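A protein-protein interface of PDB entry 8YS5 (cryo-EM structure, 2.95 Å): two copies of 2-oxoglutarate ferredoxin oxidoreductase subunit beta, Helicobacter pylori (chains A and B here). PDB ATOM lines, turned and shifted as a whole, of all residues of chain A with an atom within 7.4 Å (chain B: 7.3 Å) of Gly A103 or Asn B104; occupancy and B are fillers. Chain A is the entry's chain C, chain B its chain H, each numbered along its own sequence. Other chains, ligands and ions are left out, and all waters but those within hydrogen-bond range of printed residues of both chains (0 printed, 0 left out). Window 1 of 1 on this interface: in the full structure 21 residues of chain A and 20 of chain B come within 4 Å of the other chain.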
ATOM      1  N   GLY A  71     -33.029  15.485  22.343  1.00  0.00           N
ATOM      2  CA  GLY A  71     -31.890  16.341  22.593  1.00  0.00           C
ATOM      3  C   GLY A  71     -31.254  16.208  23.957  1.00  0.00           C
ATOM      4  O   GLY A  71     -30.236  16.865  24.210  1.00  0.00           O
ATOM      5  N   ASP A  97     -31.303  15.798  16.492  1.00  0.00           N
ATOM      6  CA  ASP A  97     -30.929  15.705  17.895  1.00  0.00           C
ATOM      7  C   ASP A  97     -29.819  16.701  18.192  1.00  0.00           C
ATOM      8  O   ASP A  97     -29.670  17.700  17.480  1.00  0.00           O
ATOM      9  CB  ASP A  97     -30.505  14.284  18.260  1.00  0.00           C
ATOM     10  CG  ASP A  97     -31.615  13.504  18.933  1.00  0.00           C
ATOM     11  OD1 ASP A  97     -32.794  13.733  18.591  1.00  0.00           O
ATOM     12  OD2 ASP A  97     -31.313  12.669  19.811  1.00  0.00           O
ATOM     13  N   GLY A  98     -29.038  16.438  19.234  1.00  0.00           N
ATOM     14  CA  GLY A  98     -28.198  17.415  19.902  1.00  0.00           C
ATOM     15  C   GLY A  98     -27.370  18.380  19.073  1.00  0.00           C
ATOM     16  O   GLY A  98     -26.664  19.212  19.645  1.00  0.00           O
ATOM     17  N   PHE A  99     -27.385  18.268  17.749  1.00  0.00           N
ATOM     18  CA  PHE A  99     -26.864  19.343  16.913  1.00  0.00           C
ATOM     19  C   PHE A  99     -27.943  20.285  16.395  1.00  0.00           C
ATOM     20  O   PHE A  99     -27.617  21.245  15.689  1.00  0.00           O
ATOM     21  CB  PHE A  99     -26.061  18.776  15.741  1.00  0.00           C
ATOM     22  CG  PHE A  99     -24.584  18.954  15.897  1.00  0.00           C
ATOM     23  CD1 PHE A  99     -24.055  20.207  16.143  1.00  0.00           C
ATOM     24  CD2 PHE A  99     -23.727  17.874  15.831  1.00  0.00           C
ATOM     25  CE1 PHE A  99     -22.698  20.383  16.296  1.00  0.00           C
ATOM     26  CE2 PHE A  99     -22.371  18.043  15.989  1.00  0.00           C
ATOM     27  N   ALA A 100     -29.213  20.045  16.723  1.00  0.00           N
ATOM     28  CA  ALA A 100     -30.290  20.959  16.354  1.00  0.00           C
ATOM     29  C   ALA A 100     -30.984  21.552  17.572  1.00  0.00           C
ATOM     30  O   ALA A 100     -31.065  22.778  17.692  1.00  0.00           O
ATOM     31  CB  ALA A 100     -31.306  20.244  15.454  1.00  0.00           C
ATOM     32  N   ILE A 101     -31.486  20.720  18.484  1.00  0.00           N
ATOM     33  CA  ILE A 101     -32.225  21.197  19.647  1.00  0.00           C
ATOM     34  C   ILE A 101     -31.327  21.140  20.874  1.00  0.00           C
ATOM     35  O   ILE A 101     -31.402  22.002  21.758  1.00  0.00           O
ATOM     36  CB  ILE A 101     -33.513  20.376  19.856  1.00  0.00           C
ATOM     37  CG1 ILE A 101     -34.149  20.690  21.211  1.00  0.00           C
ATOM     38  CG2 ILE A 101     -33.227  18.893  19.731  1.00  0.00           C
ATOM     39  CD1 ILE A 101     -35.609  20.316  21.298  1.00  0.00           C
ATOM     40  N   GLY A 102     -30.455  20.138  20.928  1.00  0.00           N
ATOM     41  CA  GLY A 102     -29.560  19.983  22.056  1.00  0.00           C
ATOM     42  C   GLY A 102     -28.164  20.498  21.786  1.00  0.00           C
ATOM     43  O   GLY A 102     -27.187  19.957  22.311  1.00  0.00           O
ATOM     44  N   GLY A 103     -28.056  21.543  20.959  1.00  0.00           N
ATOM     45  CA  GLY A 103     -26.747  22.080  20.620  1.00  0.00           C
ATOM     46  C   GLY A 103     -25.957  22.518  21.837  1.00  0.00           C
ATOM     47  O   GLY A 103     -24.744  22.303  21.914  1.00  0.00           O
ATOM     48  N   ASN A 104     -26.635  23.131  22.808  1.00  0.00           N
ATOM     49  CA  ASN A 104     -25.959  23.552  24.029  1.00  0.00           C
ATOM     50  C   ASN A 104     -25.390  22.358  24.782  1.00  0.00           C
ATOM     51  O   ASN A 104     -24.262  22.413  25.287  1.00  0.00           O
ATOM     52  CB  ASN A 104     -26.925  24.337  24.914  1.00  0.00           C
ATOM     53  CG  ASN A 104     -26.261  25.510  25.600  1.00  0.00           C
ATOM     54  OD1 ASN A 104     -25.175  25.938  25.211  1.00  0.00           O
ATOM     55  ND2 ASN A 104     -26.909  26.036  26.631  1.00  0.00           N
ATOM     56  N   HIS A 105     -26.155  21.268  24.870  1.00  0.00           N
ATOM     57  CA  HIS A 105     -25.691  20.093  25.601  1.00  0.00           C
ATOM     58  C   HIS A 105     -24.446  19.502  24.953  1.00  0.00           C
ATOM     59  O   HIS A 105     -23.471  19.174  25.639  1.00  0.00           O
ATOM     60  CB  HIS A 105     -26.804  19.049  25.675  1.00  0.00           C
ATOM     61  CG  HIS A 105     -28.101  19.585  26.197  1.00  0.00           C
ATOM     62  ND1 HIS A 105     -28.172  20.673  27.037  1.00  0.00           N
ATOM     63  CD2 HIS A 105     -29.377  19.179  25.999  1.00  0.00           C
ATOM     64  CE1 HIS A 105     -29.437  20.920  27.330  1.00  0.00           C
ATOM     65  NE2 HIS A 105     -30.187  20.025  26.713  1.00  0.00           N
ATOM     66  N   THR A 106     -24.457  19.366  23.623  1.00  0.00           N
ATOM     67  CA  THR A 106     -23.296  18.821  22.926  1.00  0.00           C
ATOM     68  C   THR A 106     -22.089  19.740  23.063  1.00  0.00           C
ATOM     69  O   THR A 106     -20.967  19.273  23.294  1.00  0.00           O
ATOM     70  CB  THR A 106     -23.627  18.589  21.452  1.00  0.00           C
ATOM     71  OG1 THR A 106     -24.921  17.984  21.341  1.00  0.00           O
ATOM     72  CG2 THR A 106     -22.596  17.676  20.815  1.00  0.00           C
ATOM     73  N   MET A 107     -22.299  21.052  22.925  1.00  0.00           N
ATOM     74  CA  MET A 107     -21.188  21.990  23.051  1.00  0.00           C
ATOM     75  C   MET A 107     -20.572  21.931  24.442  1.00  0.00           C
ATOM     76  O   MET A 107     -19.344  21.917  24.587  1.00  0.00           O
ATOM     77  CB  MET A 107     -21.659  23.409  22.734  1.00  0.00           C
ATOM     78  CG  MET A 107     -21.902  23.665  21.256  1.00  0.00           C
ATOM     79  SD  MET A 107     -20.588  23.004  20.215  1.00  0.00           S
ATOM     80  CE  MET A 107     -21.475  21.734  19.321  1.00  0.00           C
ATOM     81  N   HIS A 108     -21.405  21.875  25.483  1.00  0.00           N
ATOM     82  CA  HIS A 108     -20.872  21.842  26.839  1.00  0.00           C
ATOM     83  C   HIS A 108     -20.222  20.502  27.158  1.00  0.00           C
ATOM     84  O   HIS A 108     -19.233  20.457  27.902  1.00  0.00           O
ATOM     85  CB  HIS A 108     -21.977  22.168  27.839  1.00  0.00           C
ATOM     86  CG  HIS A 108     -22.288  23.629  27.932  1.00  0.00           C
ATOM     87  ND1 HIS A 108     -21.669  24.466  28.837  1.00  0.00           N
ATOM     88  CD2 HIS A 108     -23.141  24.408  27.227  1.00  0.00           C
ATOM     89  CE1 HIS A 108     -22.133  25.693  28.689  1.00  0.00           C
ATOM     90  NE2 HIS A 108     -23.028  25.685  27.717  1.00  0.00           N
ATOM     91  N   ALA A 109     -20.752  19.404  26.610  1.00  0.00           N
ATOM     92  CA  ALA A 109     -20.102  18.110  26.777  1.00  0.00           C
ATOM     93  C   ALA A 109     -18.726  18.104  26.127  1.00  0.00           C
ATOM     94  O   ALA A 109     -17.769  17.554  26.685  1.00  0.00           O
ATOM     95  CB  ALA A 109     -20.977  17.002  26.194  1.00  0.00           C
ATOM     96  N   PHE A 155     -24.225  23.726   8.862  1.00  0.00           N
ATOM     97  CA  PHE A 155     -23.303  23.567   9.972  1.00  0.00           C
ATOM     98  C   PHE A 155     -22.108  22.722   9.548  1.00  0.00           C
ATOM     99  O   PHE A 155     -22.123  22.046   8.517  1.00  0.00           O
ATOM    100  CB  PHE A 155     -23.994  22.919  11.173  1.00  0.00           C
ATOM    101  CG  PHE A 155     -24.440  23.898  12.219  1.00  0.00           C
ATOM    102  CD1 PHE A 155     -23.612  24.933  12.618  1.00  0.00           C
ATOM    103  CD2 PHE A 155     -25.680  23.771  12.819  1.00  0.00           C
ATOM    104  CE1 PHE A 155     -24.020  25.833  13.583  1.00  0.00           C
ATOM    105  CE2 PHE A 155     -26.091  24.665  13.787  1.00  0.00           C
ATOM    106  CZ  PHE A 155     -25.260  25.696  14.168  1.00  0.00           C
ATOM    107  N   LEU A 160     -17.270  22.551  14.246  1.00  0.00           N
ATOM    108  CA  LEU A 160     -17.941  23.081  15.427  1.00  0.00           C
ATOM    109  C   LEU A 160     -17.471  22.373  16.692  1.00  0.00           C
ATOM    110  O   LEU A 160     -17.198  23.020  17.711  1.00  0.00           O
ATOM    111  CB  LEU A 160     -19.455  22.946  15.266  1.00  0.00           C
ATOM    112  CG  LEU A 160     -20.342  23.869  16.099  1.00  0.00           C
ATOM    113  CD1 LEU A 160     -19.800  25.283  16.082  1.00  0.00           C
ATOM    114  CD2 LEU A 160     -21.765  23.838  15.580  1.00  0.00           C
ATOM    115  N   GLY B  98     -26.777  34.205  26.482  1.00  0.00           N
ATOM    116  CA  GLY B  98     -26.802  33.315  25.335  1.00  0.00           C
ATOM    117  C   GLY B  98     -25.521  32.619  24.914  1.00  0.00           C
ATOM    118  O   GLY B  98     -25.547  31.834  23.965  1.00  0.00           O
ATOM    119  N   PHE B  99     -24.390  32.908  25.552  1.00  0.00           N
ATOM    120  CA  PHE B  99     -23.211  32.066  25.383  1.00  0.00           C
ATOM    121  C   PHE B  99     -23.037  31.040  26.496  1.00  0.00           C
ATOM    122  O   PHE B  99     -22.039  30.313  26.493  1.00  0.00           O
ATOM    123  CB  PHE B  99     -21.946  32.917  25.258  1.00  0.00           C
ATOM    124  CG  PHE B  99     -21.331  32.869  23.891  1.00  0.00           C
ATOM    125  CD1 PHE B  99     -20.496  31.823  23.536  1.00  0.00           C
ATOM    126  CD2 PHE B  99     -21.599  33.852  22.957  1.00  0.00           C
ATOM    127  CE1 PHE B  99     -19.932  31.764  22.280  1.00  0.00           C
ATOM    128  CE2 PHE B  99     -21.037  33.797  21.698  1.00  0.00           C
ATOM    129  N   ALA B 100     -23.970  30.960  27.444  1.00  0.00           N
ATOM    130  CA  ALA B 100     -23.946  29.920  28.465  1.00  0.00           C
ATOM    131  C   ALA B 100     -25.177  29.030  28.427  1.00  0.00           C
ATOM    132  O   ALA B 100     -25.048  27.804  28.353  1.00  0.00           O
ATOM    133  CB  ALA B 100     -23.801  30.544  29.861  1.00  0.00           C
ATOM    134  N   ILE B 101     -26.372  29.613  28.472  1.00  0.00           N
ATOM    135  CA  ILE B 101     -27.612  28.851  28.458  1.00  0.00           C
ATOM    136  C   ILE B 101     -28.279  28.886  27.089  1.00  0.00           C
ATOM    137  O   ILE B 101     -28.770  27.862  26.611  1.00  0.00           O
ATOM    138  CB  ILE B 101     -28.568  29.366  29.559  1.00  0.00           C
ATOM    139  CG1 ILE B 101     -29.958  28.747  29.403  1.00  0.00           C
ATOM    140  CG2 ILE B 101     -28.639  30.885  29.546  1.00  0.00           C
ATOM    141  CD1 ILE B 101     -30.962  29.229  30.425  1.00  0.00           C
ATOM    142  N   GLY B 102     -28.294  30.047  26.439  1.00  0.00           N
ATOM    143  CA  GLY B 102     -28.887  30.163  25.123  1.00  0.00           C
ATOM    144  C   GLY B 102     -27.874  30.021  24.008  1.00  0.00           C
ATOM    145  O   GLY B 102     -27.941  30.743  23.009  1.00  0.00           O
ATOM    146  N   GLY B 103     -26.925  29.095  24.171  1.00  0.00           N
ATOM    147  CA  GLY B 103     -25.890  28.920  23.163  1.00  0.00           C
ATOM    148  C   GLY B 103     -26.449  28.535  21.808  1.00  0.00           C
ATOM    149  O   GLY B 103     -25.960  28.993  20.772  1.00  0.00           O
ATOM    150  N   ASN B 104     -27.485  27.696  21.799  1.00  0.00           N
ATOM    151  CA  ASN B 104     -28.080  27.265  20.540  1.00  0.00           C
ATOM    152  C   ASN B 104     -28.629  28.452  19.757  1.00  0.00           C
ATOM    153  O   ASN B 104     -28.480  28.516  18.531  1.00  0.00           O
ATOM    154  CB  ASN B 104     -29.182  26.242  20.808  1.00  0.00           C
ATOM    155  CG  ASN B 104     -29.142  25.079  19.841  1.00  0.00           C
ATOM    156  OD1 ASN B 104     -28.103  24.779  19.255  1.00  0.00           O
ATOM    157  ND2 ASN B 104     -30.276  24.412  19.670  1.00  0.00           N
ATOM    158  N   HIS B 105     -29.261  29.401  20.450  1.00  0.00           N
ATOM    159  CA  HIS B 105     -29.817  30.568  19.772  1.00  0.00           C
ATOM    160  C   HIS B 105     -28.722  31.365  19.075  1.00  0.00           C
ATOM    161  O   HIS B 105     -28.857  31.732  17.903  1.00  0.00           O
ATOM    162  CB  HIS B 105     -30.561  31.451  20.773  1.00  0.00           C
ATOM    163  CG  HIS B 105     -31.484  30.696  21.678  1.00  0.00           C
ATOM    164  ND1 HIS B 105     -32.114  29.531  21.300  1.00  0.00           N
ATOM    165  CD2 HIS B 105     -31.883  30.944  22.949  1.00  0.00           C
ATOM    166  CE1 HIS B 105     -32.858  29.091  22.299  1.00  0.00           C
ATOM    167  NE2 HIS B 105     -32.738  29.931  23.310  1.00  0.00           N
ATOM    168  N   THR B 106     -27.622  31.632  19.783  1.00  0.00           N
ATOM    169  CA  THR B 106     -26.527  32.394  19.193  1.00  0.00           C
ATOM    170  C   THR B 106     -25.899  31.650  18.022  1.00  0.00           C
ATOM    171  O   THR B 106     -25.626  32.247  16.973  1.00  0.00           O
ATOM    172  CB  THR B 106     -25.469  32.705  20.252  1.00  0.00           C
ATOM    173  OG1 THR B 106     -26.099  33.271  21.407  1.00  0.00           O
ATOM    174  CG2 THR B 106     -24.446  33.688  19.707  1.00  0.00           C
ATOM    175  N   MET B 107     -25.663  30.343  18.178  1.00  0.00           N
ATOM    176  CA  MET B 107     -25.032  29.587  17.102  1.00  0.00           C
ATOM    177  C   MET B 107     -25.915  29.549  15.861  1.00  0.00           C
ATOM    178  O   MET B 107     -25.425  29.715  14.738  1.00  0.00           O
ATOM    179  CB  MET B 107     -24.700  28.170  17.568  1.00  0.00           C
ATOM    180  CG  MET B 107     -23.792  28.126  18.780  1.00  0.00           C
ATOM    181  SD  MET B 107     -22.426  29.294  18.667  1.00  0.00           S
ATOM    182  CE  MET B 107     -21.851  29.278  20.361  1.00  0.00           C
ATOM    183  N   HIS B 108     -27.222  29.354  16.039  1.00  0.00           N
ATOM    184  CA  HIS B 108     -28.103  29.293  14.880  1.00  0.00           C
ATOM    185  C   HIS B 108     -28.299  30.664  14.244  1.00  0.00           C
ATOM    186  O   HIS B 108     -28.429  30.760  13.019  1.00  0.00           O
ATOM    187  CB  HIS B 108     -29.441  28.671  15.273  1.00  0.00           C
ATOM    188  CG  HIS B 108     -29.387  27.182  15.414  1.00  0.00           C
ATOM    189  ND1 HIS B 108     -29.624  26.326  14.362  1.00  0.00           N
ATOM    190  CD2 HIS B 108     -29.111  26.397  16.482  1.00  0.00           C
ATOM    191  CE1 HIS B 108     -29.503  25.078  14.775  1.00  0.00           C
ATOM    192  NE2 HIS B 108     -29.193  25.093  16.059  1.00  0.00           N
ATOM    193  N   ALA B 109     -28.312  31.732  15.048  1.00  0.00           N
ATOM    194  CA  ALA B 109     -28.366  33.076  14.480  1.00  0.00           C
ATOM    195  C   ALA B 109     -27.112  33.375  13.672  1.00  0.00           C
ATOM    196  O   ALA B 109     -27.182  34.017  12.617  1.00  0.00           O
ATOM    197  CB  ALA B 109     -28.553  34.110  15.588  1.00  0.00           C
ATOM    198  N   CYS B 110     -25.952  32.928  14.158  1.00  0.00           N
ATOM    199  CA  CYS B 110     -24.730  33.039  13.369  1.00  0.00           C
ATOM    200  C   CYS B 110     -24.843  32.243  12.075  1.00  0.00           C
ATOM    201  O   CYS B 110     -24.423  32.708  11.010  1.00  0.00           O
ATOM    202  CB  CYS B 110     -23.530  32.556  14.183  1.00  0.00           C
ATOM    203  SG  CYS B 110     -22.989  33.680  15.484  1.00  0.00           S
ATOM    204  N   ARG B 112     -27.556  31.267  10.268  1.00  0.00           N
ATOM    205  CA  ARG B 112     -28.478  31.764   9.252  1.00  0.00           C
ATOM    206  C   ARG B 112     -28.218  33.212   8.857  1.00  0.00           C
ATOM    207  O   ARG B 112     -28.858  33.698   7.918  1.00  0.00           O
ATOM    208  CB  ARG B 112     -29.930  31.606   9.716  1.00  0.00           C
ATOM    209  CG  ARG B 112     -30.267  32.298  11.017  1.00  0.00           C
ATOM    210  CD  ARG B 112     -31.759  32.221  11.294  1.00  0.00           C
ATOM    211  NE  ARG B 112     -32.236  30.844  11.332  1.00  0.00           N
ATOM    212  CZ  ARG B 112     -32.539  30.184  12.441  1.00  0.00           C
ATOM    213  NH1 ARG B 112     -32.417  30.745  13.634  1.00  0.00           N
ATOM    214  NH2 ARG B 112     -32.975  28.931  12.353  1.00  0.00           N
ATOM    215  N   PHE B 155     -14.600  28.206  26.863  1.00  0.00           N
ATOM    216  CA  PHE B 155     -15.153  28.481  25.549  1.00  0.00           C
ATOM    217  C   PHE B 155     -14.402  29.639  24.905  1.00  0.00           C
ATOM    218  O   PHE B 155     -13.874  30.522  25.587  1.00  0.00           O
ATOM    219  CB  PHE B 155     -16.642  28.823  25.634  1.00  0.00           C
ATOM    220  CG  PHE B 155     -17.551  27.650  25.410  1.00  0.00           C
ATOM    221  CD1 PHE B 155     -17.430  26.871  24.276  1.00  0.00           C
ATOM    222  CD2 PHE B 155     -18.555  27.353  26.314  1.00  0.00           C
ATOM    223  CE1 PHE B 155     -18.272  25.795  24.064  1.00  0.00           C
ATOM    224  CE2 PHE B 155     -19.402  26.284  26.105  1.00  0.00           C
ATOM    225  CZ  PHE B 155     -19.261  25.505  24.978  1.00  0.00           C
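The backbone carbonyl oxygen (O) of Ala A100 lies within hydrogen-bond range of the side-chain amide nitrogen (ND2) of Asn B104 (2.7 Å).
The backbone carbonyl oxygen (O) of Ala A100 sits at hydrogen-bond distance from a ring nitrogen (NE2) of His B108.
The backbone carbonyl oxygen (O) of Ile A101 sits at hydrogen-bond distance from the side-chain amide nitrogen (ND2) of Asn B104 (3.4 Å).
ND2 of Asn A104 lies within hydrogen-bond range of O of Ala B100, at 3.1 Å.
The backbone carbonyl oxygen (O) of Ile B101 sits at hydrogen-bond distance from the side-chain amide nitrogen (ND2) of Asn A104 (2.6 Å).
NE2 of His A108 sits at hydrogen-bond distance from O of Ala B100, at 3.0 Å.
The backbone carbonyl oxygen (O) of Gly A98 sits at hydrogen-bond distance from the backbone NH (N) of Gly A103 (3.0 Å).
A ring nitrogen (NE2) of His A108 sits close to the side-chain amide oxygen (OD1) of Asn A104.
O of Gly B98 sits close to N of Gly B103.
The side-chain amide oxygen of Asn B104 sits close to a ring nitrogen (NE2) of His B108.
CA of Gly A103 touches OD1 of Asn B104, at 3.3 Å.
Asn A104 touches Gly B103 (OD1 to CA, 3.7 Å).
Phe B155 touches Met A107.
CE1 of His A108 touches CE2 of Phe B155 (3.8 Å).
CE2 of Phe A155 touches CE1 of His B108, at 3.6 Å.
Of the printed residues of chain B, Ile A101 touches Asn B104.
No residue of chain B comes within 4 Å of Gly A102.
Gly A103 touches just one residue of chain B: Asn B104 (3.3 Å).
Of the printed residues of chain B, His A108 touches Ala B100 (3.0 Å) and Phe B155 (3.8 Å).
Leu A160 touches none of the printed residues of chain B.
Gly B103 touches just one residue of chain A: Asn A104 (3.7 Å).
Of chain A, only Ala A100, Ile A101 and Gly A103 come within 4 Å of Asn B104.
Thr B106 touches none of the printed residues of chain A.
Of the printed residues of chain A, His B108 touches Ala A100 (3.4 Å) and Phe A155 (3.6 Å).
The nearest printed residue of chain B that does not touch Asn A104 is Asn B104 (4.2 Å).
Of the 15 printed residues of chain B, 6 touch a printed residue of chain A.
Hydrophobic or aromatic side chains of chain B within 4 Å of the printed part of chain A: His B108 and Phe B155.
Along chain B the printed residues that touch a printed residue of chain A span positions 100 to 155.
Of the 16 printed residues of chain A, 7 touch a printed residue of chain B.
Hydrophobic or aromatic side chains of chain A within 4 Å of the printed part of chain B: Met A107, His A108 and Phe A155.
Among the printed residues, 11 pairs touch across the chains.
Ala A100 touches Asn B104, and with the chains exchanged Asn A104 touches Ala B100.
Ala A100 touches His B108, and with the chains exchanged His A108 touches Ala B100.
Gly A103 touches Asn B104, and with the chains exchanged Asn A104 touches Gly B103.
Met A107 touches Phe B155, but with the chains exchanged Phe A155 does not touch Met B107 (4.1 Å).
13 positions are printed for both chains.
Of the 11 pairs that touch across the chains among the printed residues, 10 have their exchanged pair printed and touching as well.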
